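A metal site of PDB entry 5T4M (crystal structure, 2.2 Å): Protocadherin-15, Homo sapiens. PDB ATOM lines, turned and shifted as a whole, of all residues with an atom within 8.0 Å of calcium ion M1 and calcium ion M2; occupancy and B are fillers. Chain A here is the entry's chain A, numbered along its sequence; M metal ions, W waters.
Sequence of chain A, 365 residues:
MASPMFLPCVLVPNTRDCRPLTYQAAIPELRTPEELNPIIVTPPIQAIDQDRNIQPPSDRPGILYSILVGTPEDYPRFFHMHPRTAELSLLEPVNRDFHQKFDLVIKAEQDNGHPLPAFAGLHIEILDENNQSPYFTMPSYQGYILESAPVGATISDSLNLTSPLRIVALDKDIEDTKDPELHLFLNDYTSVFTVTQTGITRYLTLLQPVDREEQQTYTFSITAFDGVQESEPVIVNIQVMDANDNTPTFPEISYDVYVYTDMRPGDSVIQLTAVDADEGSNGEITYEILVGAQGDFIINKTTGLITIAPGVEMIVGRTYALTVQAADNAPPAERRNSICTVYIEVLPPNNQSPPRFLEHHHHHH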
ATOM      1  N   GLU A  29      16.136   1.959  18.423  1.00  0.00           N
ATOM      2  CA  GLU A  29      15.157   2.603  17.562  1.00  0.00           C
ATOM      3  C   GLU A  29      13.753   2.015  17.764  1.00  0.00           C
ATOM      4  O   GLU A  29      13.596   0.808  17.898  1.00  0.00           O
ATOM      5  CB  GLU A  29      15.577   2.454  16.094  1.00  0.00           C
ATOM      6  CG  GLU A  29      14.528   2.899  15.083  1.00  0.00           C
ATOM      7  CD  GLU A  29      14.763   2.303  13.712  1.00  0.00           C
ATOM      8  OE1 GLU A  29      15.292   1.181  13.626  1.00  0.00           O
ATOM      9  OE2 GLU A  29      14.419   2.974  12.711  1.00  0.00           O
ATOM     10  N   ARG A  96      15.250   5.970  13.416  1.00  0.00           N
ATOM     11  CA  ARG A  96      16.635   6.189  13.036  1.00  0.00           C
ATOM     12  C   ARG A  96      16.770   6.776  11.635  1.00  0.00           C
ATOM     13  O   ARG A  96      17.797   7.379  11.313  1.00  0.00           O
ATOM     14  CB  ARG A  96      17.434   4.886  13.127  1.00  0.00           C
ATOM     15  CG  ARG A  96      18.930   5.117  13.207  1.00  0.00           C
ATOM     16  CD  ARG A  96      19.722   3.830  13.314  1.00  0.00           C
ATOM     17  NE  ARG A  96      21.139   4.112  13.505  1.00  0.00           N
ATOM     18  CZ  ARG A  96      21.980   4.403  12.521  1.00  0.00           C
ATOM     19  NH1 ARG A  96      21.563   4.425  11.266  1.00  0.00           N
ATOM     20  NH2 ARG A  96      23.256   4.659  12.789  1.00  0.00           N
ATOM     21  N   LEU A 127      20.163   3.303  17.946  1.00  0.00           N
ATOM     22  CA  LEU A 127      20.634   2.006  17.466  1.00  0.00           C
ATOM     23  C   LEU A 127      19.732   1.375  16.408  1.00  0.00           C
ATOM     24  O   LEU A 127      18.508   1.385  16.543  1.00  0.00           O
ATOM     25  CB  LEU A 127      20.772   1.036  18.646  1.00  0.00           C
ATOM     26  CG  LEU A 127      21.717   1.424  19.777  1.00  0.00           C
ATOM     27  CD1 LEU A 127      21.563   0.458  20.949  1.00  0.00           C
ATOM     28  CD2 LEU A 127      23.164   1.462  19.300  1.00  0.00           C
ATOM     29  N   ASP A 128      20.354   0.838  15.367  1.00  0.00           N
ATOM     30  CA  ASP A 128      19.658  -0.068  14.448  1.00  0.00           C
ATOM     31  C   ASP A 128      19.259  -1.306  15.238  1.00  0.00           C
ATOM     32  O   ASP A 128      19.941  -1.709  16.174  1.00  0.00           O
ATOM     33  CB  ASP A 128      20.550  -0.453  13.259  1.00  0.00           C
ATOM     34  CG  ASP A 128      20.397   0.482  12.079  1.00  0.00           C
ATOM     35  OD1 ASP A 128      19.246   0.729  11.664  1.00  0.00           O
ATOM     36  OD2 ASP A 128      21.425   0.977  11.571  1.00  0.00           O
ATOM     37  N   GLU A 129      18.143  -1.913  14.862  1.00  0.00           N
ATOM     38  CA  GLU A 129      17.680  -3.114  15.543  1.00  0.00           C
ATOM     39  C   GLU A 129      17.223  -4.181  14.554  1.00  0.00           C
ATOM     40  O   GLU A 129      16.840  -3.880  13.427  1.00  0.00           O
ATOM     41  CB  GLU A 129      16.529  -2.774  16.511  1.00  0.00           C
ATOM     42  CG  GLU A 129      16.927  -1.879  17.673  1.00  0.00           C
ATOM     43  CD  GLU A 129      17.921  -2.540  18.617  1.00  0.00           C
ATOM     44  OE1 GLU A 129      17.925  -3.790  18.713  1.00  0.00           O
ATOM     45  OE2 GLU A 129      18.699  -1.811  19.279  1.00  0.00           O
ATOM     46  N   ASN A 130      17.292  -5.434  15.003  1.00  0.00           N
ATOM     47  CA  ASN A 130      16.755  -6.552  14.237  1.00  0.00           C
ATOM     48  C   ASN A 130      15.239  -6.495  14.262  1.00  0.00           C
ATOM     49  O   ASN A 130      14.597  -7.241  14.999  1.00  0.00           O
ATOM     50  CB  ASN A 130      17.252  -7.885  14.815  1.00  0.00           C
ATOM     51  CG  ASN A 130      16.867  -9.079  13.947  1.00  0.00           C
ATOM     52  OD1 ASN A 130      15.968  -9.007  13.103  1.00  0.00           O
ATOM     53  ND2 ASN A 130      17.537 -10.198  14.178  1.00  0.00           N
ATOM     54  N   ASN A 131      14.665  -5.600  13.460  1.00  0.00           N
ATOM     55  CA  ASN A 131      13.235  -5.327  13.514  1.00  0.00           C
ATOM     56  C   ASN A 131      12.522  -5.582  12.192  1.00  0.00           C
ATOM     57  O   ASN A 131      11.406  -5.109  11.978  1.00  0.00           O
ATOM     58  CB  ASN A 131      12.990  -3.883  13.981  1.00  0.00           C
ATOM     59  CG  ASN A 131      13.950  -2.893  13.325  1.00  0.00           C
ATOM     60  OD1 ASN A 131      14.529  -3.158  12.275  1.00  0.00           O
ATOM     61  ND2 ASN A 131      14.117  -1.735  13.963  1.00  0.00           N
ATOM     62  N   GLN A 132      13.170  -6.322  11.305  1.00  0.00           N
ATOM     63  CA  GLN A 132      12.546  -6.723  10.039  1.00  0.00           C
ATOM     64  C   GLN A 132      12.485  -8.245   9.957  1.00  0.00           C
ATOM     65  O   GLN A 132      13.483  -8.935  10.160  1.00  0.00           O
ATOM     66  CB  GLN A 132      13.327  -6.159   8.850  1.00  0.00           C
ATOM     67  CG  GLN A 132      13.474  -4.639   8.836  1.00  0.00           C
ATOM     68  CD  GLN A 132      12.198  -3.913   8.454  1.00  0.00           C
ATOM     69  OE1 GLN A 132      11.554  -4.242   7.459  1.00  0.00           O
ATOM     70  NE2 GLN A 132      11.828  -2.926   9.255  1.00  0.00           N
ATOM     71  N   SER A 133      11.296  -8.774   9.661  1.00  0.00           N
ATOM     72  CA  SER A 133      11.127 -10.220   9.505  1.00  0.00           C
ATOM     73  C   SER A 133      11.815 -10.704   8.238  1.00  0.00           C
ATOM     74  O   SER A 133      11.734 -10.053   7.194  1.00  0.00           O
ATOM     75  CB  SER A 133       9.644 -10.588   9.465  1.00  0.00           C
ATOM     76  OG  SER A 133       8.994 -10.275  10.692  1.00  0.00           O
ATOM     77  N   PRO A 134      12.493 -11.858   8.323  1.00  0.00           N
ATOM     78  CA  PRO A 134      13.065 -12.451   7.114  1.00  0.00           C
ATOM     79  C   PRO A 134      11.954 -12.890   6.151  1.00  0.00           C
ATOM     80  O   PRO A 134      10.787 -12.923   6.535  1.00  0.00           O
ATOM     81  CB  PRO A 134      13.850 -13.646   7.657  1.00  0.00           C
ATOM     82  CG  PRO A 134      13.171 -13.993   8.940  1.00  0.00           C
ATOM     83  CD  PRO A 134      12.725 -12.687   9.518  1.00  0.00           C
ATOM     84  N   TYR A 135      12.325 -13.202   4.919  1.00  0.00           N
ATOM     85  CA  TYR A 135      11.338 -13.561   3.911  1.00  0.00           C
ATOM     86  C   TYR A 135      11.959 -14.385   2.793  1.00  0.00           C
ATOM     87  O   TYR A 135      13.164 -14.319   2.542  1.00  0.00           O
ATOM     88  CB  TYR A 135      10.676 -12.302   3.339  1.00  0.00           C
ATOM     89  CG  TYR A 135      11.621 -11.407   2.545  1.00  0.00           C
ATOM     90  CD1 TYR A 135      12.355 -10.406   3.176  1.00  0.00           C
ATOM     91  CD2 TYR A 135      11.761 -11.561   1.170  1.00  0.00           C
ATOM     92  CE1 TYR A 135      13.215  -9.594   2.454  1.00  0.00           C
ATOM     93  CE2 TYR A 135      12.623 -10.753   0.440  1.00  0.00           C
ATOM     94  CZ  TYR A 135      13.339  -9.779   1.089  1.00  0.00           C
ATOM     95  OH  TYR A 135      14.191  -8.972   0.368  1.00  0.00           O
ATOM     96  N   LEU A 170      15.996 -13.887   2.522  1.00  0.00           N
ATOM     97  CA  LEU A 170      16.630 -12.607   2.790  1.00  0.00           C
ATOM     98  C   LEU A 170      16.061 -11.933   4.034  1.00  0.00           C
ATOM     99  O   LEU A 170      15.102 -12.434   4.629  1.00  0.00           O
ATOM    100  CB  LEU A 170      16.467 -11.678   1.579  1.00  0.00           C
ATOM    101  CG  LEU A 170      17.207 -12.091   0.315  1.00  0.00           C
ATOM    102  CD1 LEU A 170      16.998 -11.071  -0.797  1.00  0.00           C
ATOM    103  CD2 LEU A 170      18.681 -12.273   0.598  1.00  0.00           C
ATOM    104  N   ASP A 171      16.658 -10.811   4.420  1.00  0.00           N
ATOM    105  CA  ASP A 171      16.254 -10.069   5.619  1.00  0.00           C
ATOM    106  C   ASP A 171      16.723  -8.620   5.481  1.00  0.00           C
ATOM    107  O   ASP A 171      17.912  -8.359   5.295  1.00  0.00           O
ATOM    108  CB  ASP A 171      16.859 -10.713   6.881  1.00  0.00           C
ATOM    109  CG  ASP A 171      16.229 -10.205   8.178  1.00  0.00           C
ATOM    110  OD1 ASP A 171      16.043  -8.985   8.348  1.00  0.00           O
ATOM    111  OD2 ASP A 171      15.926 -11.057   9.052  1.00  0.00           O
ATOM    112  N   LYS A 172      15.778  -7.684   5.559  1.00  0.00           N
ATOM    113  CA  LYS A 172      16.076  -6.275   5.316  1.00  0.00           C
ATOM    114  C   LYS A 172      16.996  -5.638   6.363  1.00  0.00           C
ATOM    115  O   LYS A 172      17.501  -4.542   6.145  1.00  0.00           O
ATOM    116  CB  LYS A 172      14.781  -5.457   5.220  1.00  0.00           C
ATOM    117  CG  LYS A 172      14.035  -5.617   3.902  1.00  0.00           C
ATOM    118  CD  LYS A 172      14.897  -5.168   2.735  1.00  0.00           C
ATOM    119  CE  LYS A 172      14.206  -5.404   1.398  1.00  0.00           C
ATOM    120  NZ  LYS A 172      12.932  -4.644   1.283  1.00  0.00           N
ATOM    121  N   ASP A 173      17.203  -6.314   7.487  1.00  0.00           N
ATOM    122  CA  ASP A 173      18.122  -5.818   8.501  1.00  0.00           C
ATOM    123  C   ASP A 173      19.572  -6.059   8.072  1.00  0.00           C
ATOM    124  O   ASP A 173      20.487  -5.427   8.584  1.00  0.00           O
ATOM    125  CB  ASP A 173      17.858  -6.490   9.862  1.00  0.00           C
ATOM    126  CG  ASP A 173      16.547  -6.045  10.469  1.00  0.00           C
ATOM    127  OD1 ASP A 173      16.204  -4.855  10.341  1.00  0.00           O
ATOM    128  OD2 ASP A 173      15.857  -6.884  11.094  1.00  0.00           O
ATOM    129  N   ILE A 174      19.742  -6.980   7.134  1.00  0.00           N
ATOM    130  CA  ILE A 174      21.066  -7.334   6.624  1.00  0.00           C
ATOM    131  C   ILE A 174      21.293  -6.723   5.238  1.00  0.00           C
ATOM    132  O   ILE A 174      20.431  -6.818   4.364  1.00  0.00           O
ATOM    133  CB  ILE A 174      21.233  -8.870   6.535  1.00  0.00           C
ATOM    134  CG1 ILE A 174      20.845  -9.532   7.865  1.00  0.00           C
ATOM    135  CG2 ILE A 174      22.656  -9.238   6.139  1.00  0.00           C
ATOM    136  CD1 ILE A 174      21.639  -9.056   9.062  1.00  0.00           C
ATOM    137  N   PRO A 180      22.486 -13.396   5.692  1.00  0.00           N
ATOM    138  CA  PRO A 180      21.655 -13.002   6.843  1.00  0.00           C
ATOM    139  C   PRO A 180      21.739 -14.001   8.006  1.00  0.00           C
ATOM    140  O   PRO A 180      21.186 -13.738   9.070  1.00  0.00           O
ATOM    141  CB  PRO A 180      20.237 -12.960   6.254  1.00  0.00           C
ATOM    142  CG  PRO A 180      20.285 -13.919   5.120  1.00  0.00           C
ATOM    143  CD  PRO A 180      21.666 -13.803   4.541  1.00  0.00           C
ATOM    144  N   LEU A 182      20.338 -16.922   8.669  1.00  0.00           N
ATOM    145  CA  LEU A 182      19.016 -17.294   9.157  1.00  0.00           C
ATOM    146  C   LEU A 182      18.972 -18.754   9.581  1.00  0.00           C
ATOM    147  O   LEU A 182      19.735 -19.576   9.082  1.00  0.00           O
ATOM    148  CB  LEU A 182      17.965 -17.033   8.074  1.00  0.00           C
ATOM    149  CG  LEU A 182      17.879 -15.578   7.592  1.00  0.00           C
ATOM    150  CD1 LEU A 182      16.969 -15.481   6.372  1.00  0.00           C
ATOM    151  CD2 LEU A 182      17.391 -14.680   8.721  1.00  0.00           C
ATOM    152  N   PHE A 225      14.067 -17.814  10.464  1.00  0.00           N
ATOM    153  CA  PHE A 225      14.132 -17.201  11.794  1.00  0.00           C
ATOM    154  C   PHE A 225      15.445 -16.423  11.971  1.00  0.00           C
ATOM    155  O   PHE A 225      16.521 -16.956  11.687  1.00  0.00           O
ATOM    156  CB  PHE A 225      13.983 -18.268  12.875  1.00  0.00           C
ATOM    157  CG  PHE A 225      14.044 -17.738  14.277  1.00  0.00           C
ATOM    158  CD1 PHE A 225      13.118 -16.801  14.722  1.00  0.00           C
ATOM    159  CD2 PHE A 225      15.015 -18.187  15.161  1.00  0.00           C
ATOM    160  CE1 PHE A 225      13.168 -16.327  16.015  1.00  0.00           C
ATOM    161  CE2 PHE A 225      15.059 -17.702  16.460  1.00  0.00           C
ATOM    162  CZ  PHE A 225      14.136 -16.772  16.887  1.00  0.00           C
ATOM    163  N   ASP A 226      15.338 -15.178  12.423  1.00  0.00           N
ATOM    164  CA  ASP A 226      16.520 -14.305  12.516  1.00  0.00           C
ATOM    165  C   ASP A 226      16.991 -14.077  13.944  1.00  0.00           C
ATOM    166  O   ASP A 226      17.816 -13.188  14.198  1.00  0.00           O
ATOM    167  CB  ASP A 226      16.231 -12.946  11.849  1.00  0.00           C
ATOM    168  CG  ASP A 226      15.088 -12.184  12.512  1.00  0.00           C
ATOM    169  OD1 ASP A 226      14.586 -12.606  13.578  1.00  0.00           O
ATOM    170  OD2 ASP A 226      14.679 -11.139  11.956  1.00  0.00           O
ATOM    171  N   GLY A 227      16.467 -14.860  14.882  1.00  0.00           N
ATOM    172  CA  GLY A 227      16.811 -14.697  16.284  1.00  0.00           C
ATOM    173  C   GLY A 227      15.785 -13.883  17.041  1.00  0.00           C
ATOM    174  O   GLY A 227      15.785 -13.871  18.271  1.00  0.00           O
ATOM    175  N   VAL A 228      14.902 -13.205  16.320  1.00  0.00           N
ATOM    176  CA  VAL A 228      13.870 -12.379  16.943  1.00  0.00           C
ATOM    177  C   VAL A 228      12.480 -12.661  16.380  1.00  0.00           C
ATOM    178  O   VAL A 228      11.531 -12.879  17.118  1.00  0.00           O
ATOM    179  CB  VAL A 228      14.176 -10.872  16.794  1.00  0.00           C
ATOM    180  CG1 VAL A 228      13.109 -10.038  17.485  1.00  0.00           C
ATOM    181  CG2 VAL A 228      15.549 -10.543  17.349  1.00  0.00           C
ATOM    182  N   GLN A 229      12.378 -12.632  15.045  1.00  0.00           N
ATOM    183  CA  GLN A 229      11.093 -12.810  14.372  1.00  0.00           C
ATOM    184  C   GLN A 229      11.137 -13.962  13.373  1.00  0.00           C
ATOM    185  O   GLN A 229      12.178 -14.259  12.794  1.00  0.00           O
ATOM    186  CB  GLN A 229      10.672 -11.527  13.662  1.00  0.00           C
ATOM    187  CG  GLN A 229      10.497 -10.321  14.569  1.00  0.00           C
ATOM    188  CD  GLN A 229      11.592  -9.277  14.405  1.00  0.00           C
ATOM    189  OE1 GLN A 229      12.538  -9.456  13.630  1.00  0.00           O
ATOM    190  NE2 GLN A 229      11.468  -8.183  15.135  1.00  0.00           N
HETATM  191 CA    CA M   1      16.648  -2.752  11.301  1.00  0.00          CA
HETATM  192 CA    CA M   2      15.738  -9.317  10.771  1.00  0.00          CA
HETATM  193  O   HOH W   1      18.086  -9.666  10.910  1.00  0.00           O
HETATM  194  O   HOH W   2      16.939  -0.595  12.339  1.00  0.00           O
HETATM  195  O   HOH W   3      17.932  -2.129   9.298  1.00  0.00           O
HETATM  196  O   HOH W   4      15.394  -1.594   9.581  1.00  0.00           O
HETATM  197  O   HOH W   5      18.990  -3.078  11.527  1.00  0.00           O
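OD1 of Asp 226 sits at hydrogen-bond distance from N of Val 228. The side-chain carboxylate (OD1) of Asp 226 is in hydrogen-bond range of the backbone NH (N) of Gln 229 (2.7 Å). The side-chain amide nitrogen (ND2) of Asn 131 lies within hydrogen-bond range of the side-chain carboxylate (OE1) of Glu 29. O of Asn 130 sits at hydrogen-bond distance from NE2 of Gln 229.
Within 4 Å of calcium ion M1: Glu 129, Asn 131 and Asp 173.
Of the 23 residues printed, 5 come within 4 Å of calcium ion M2. The nearest printed residue that does not touch calcium ion M2 is Gln 229 (4.3 Å).
Calcium ion M1 is bound by OD1 of Asp 173 (2.4 Å), OD1 of Asn 131 (2.4 Å), water W5 (2.4 Å), water W2 (2.4 Å), O of Glu 129 (2.4 Å), water W4 (2.4 Å) and water W3 (2.5 Å). Calcium ion M1 has seven donor atoms within binding distance.
Calcium ion M2 is bound by the side-chain amide oxygen (OD1) of Asn 130, 2.4 Å away. Calcium ion M2 is bound by O of Gln 132, 2.4 Å away. Water W1 is bound to calcium ion M2 (2.4 Å). Calcium ion M2 is bound by the side-chain carboxylate (OD2) of Asp 226 (2.4 Å). The side-chain carboxylate (OD2) of Asp 171 binds calcium ion M2, at 2.5 Å. Calcium ion M2 is bound by the side-chain carboxylate (OD2) of Asp 173 (2.5 Å). The side-chain carboxylate (OD1) of Asp 171 is bound to calcium ion M2, at 2.5 Å. Calcium ion M2 has seven donor atoms within binding distance.
Water W2 lies within hydrogen-bond range of OE1 of Glu 29, OD1 of Asp 128, N of Glu 129 and ND2 of Asn 131.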
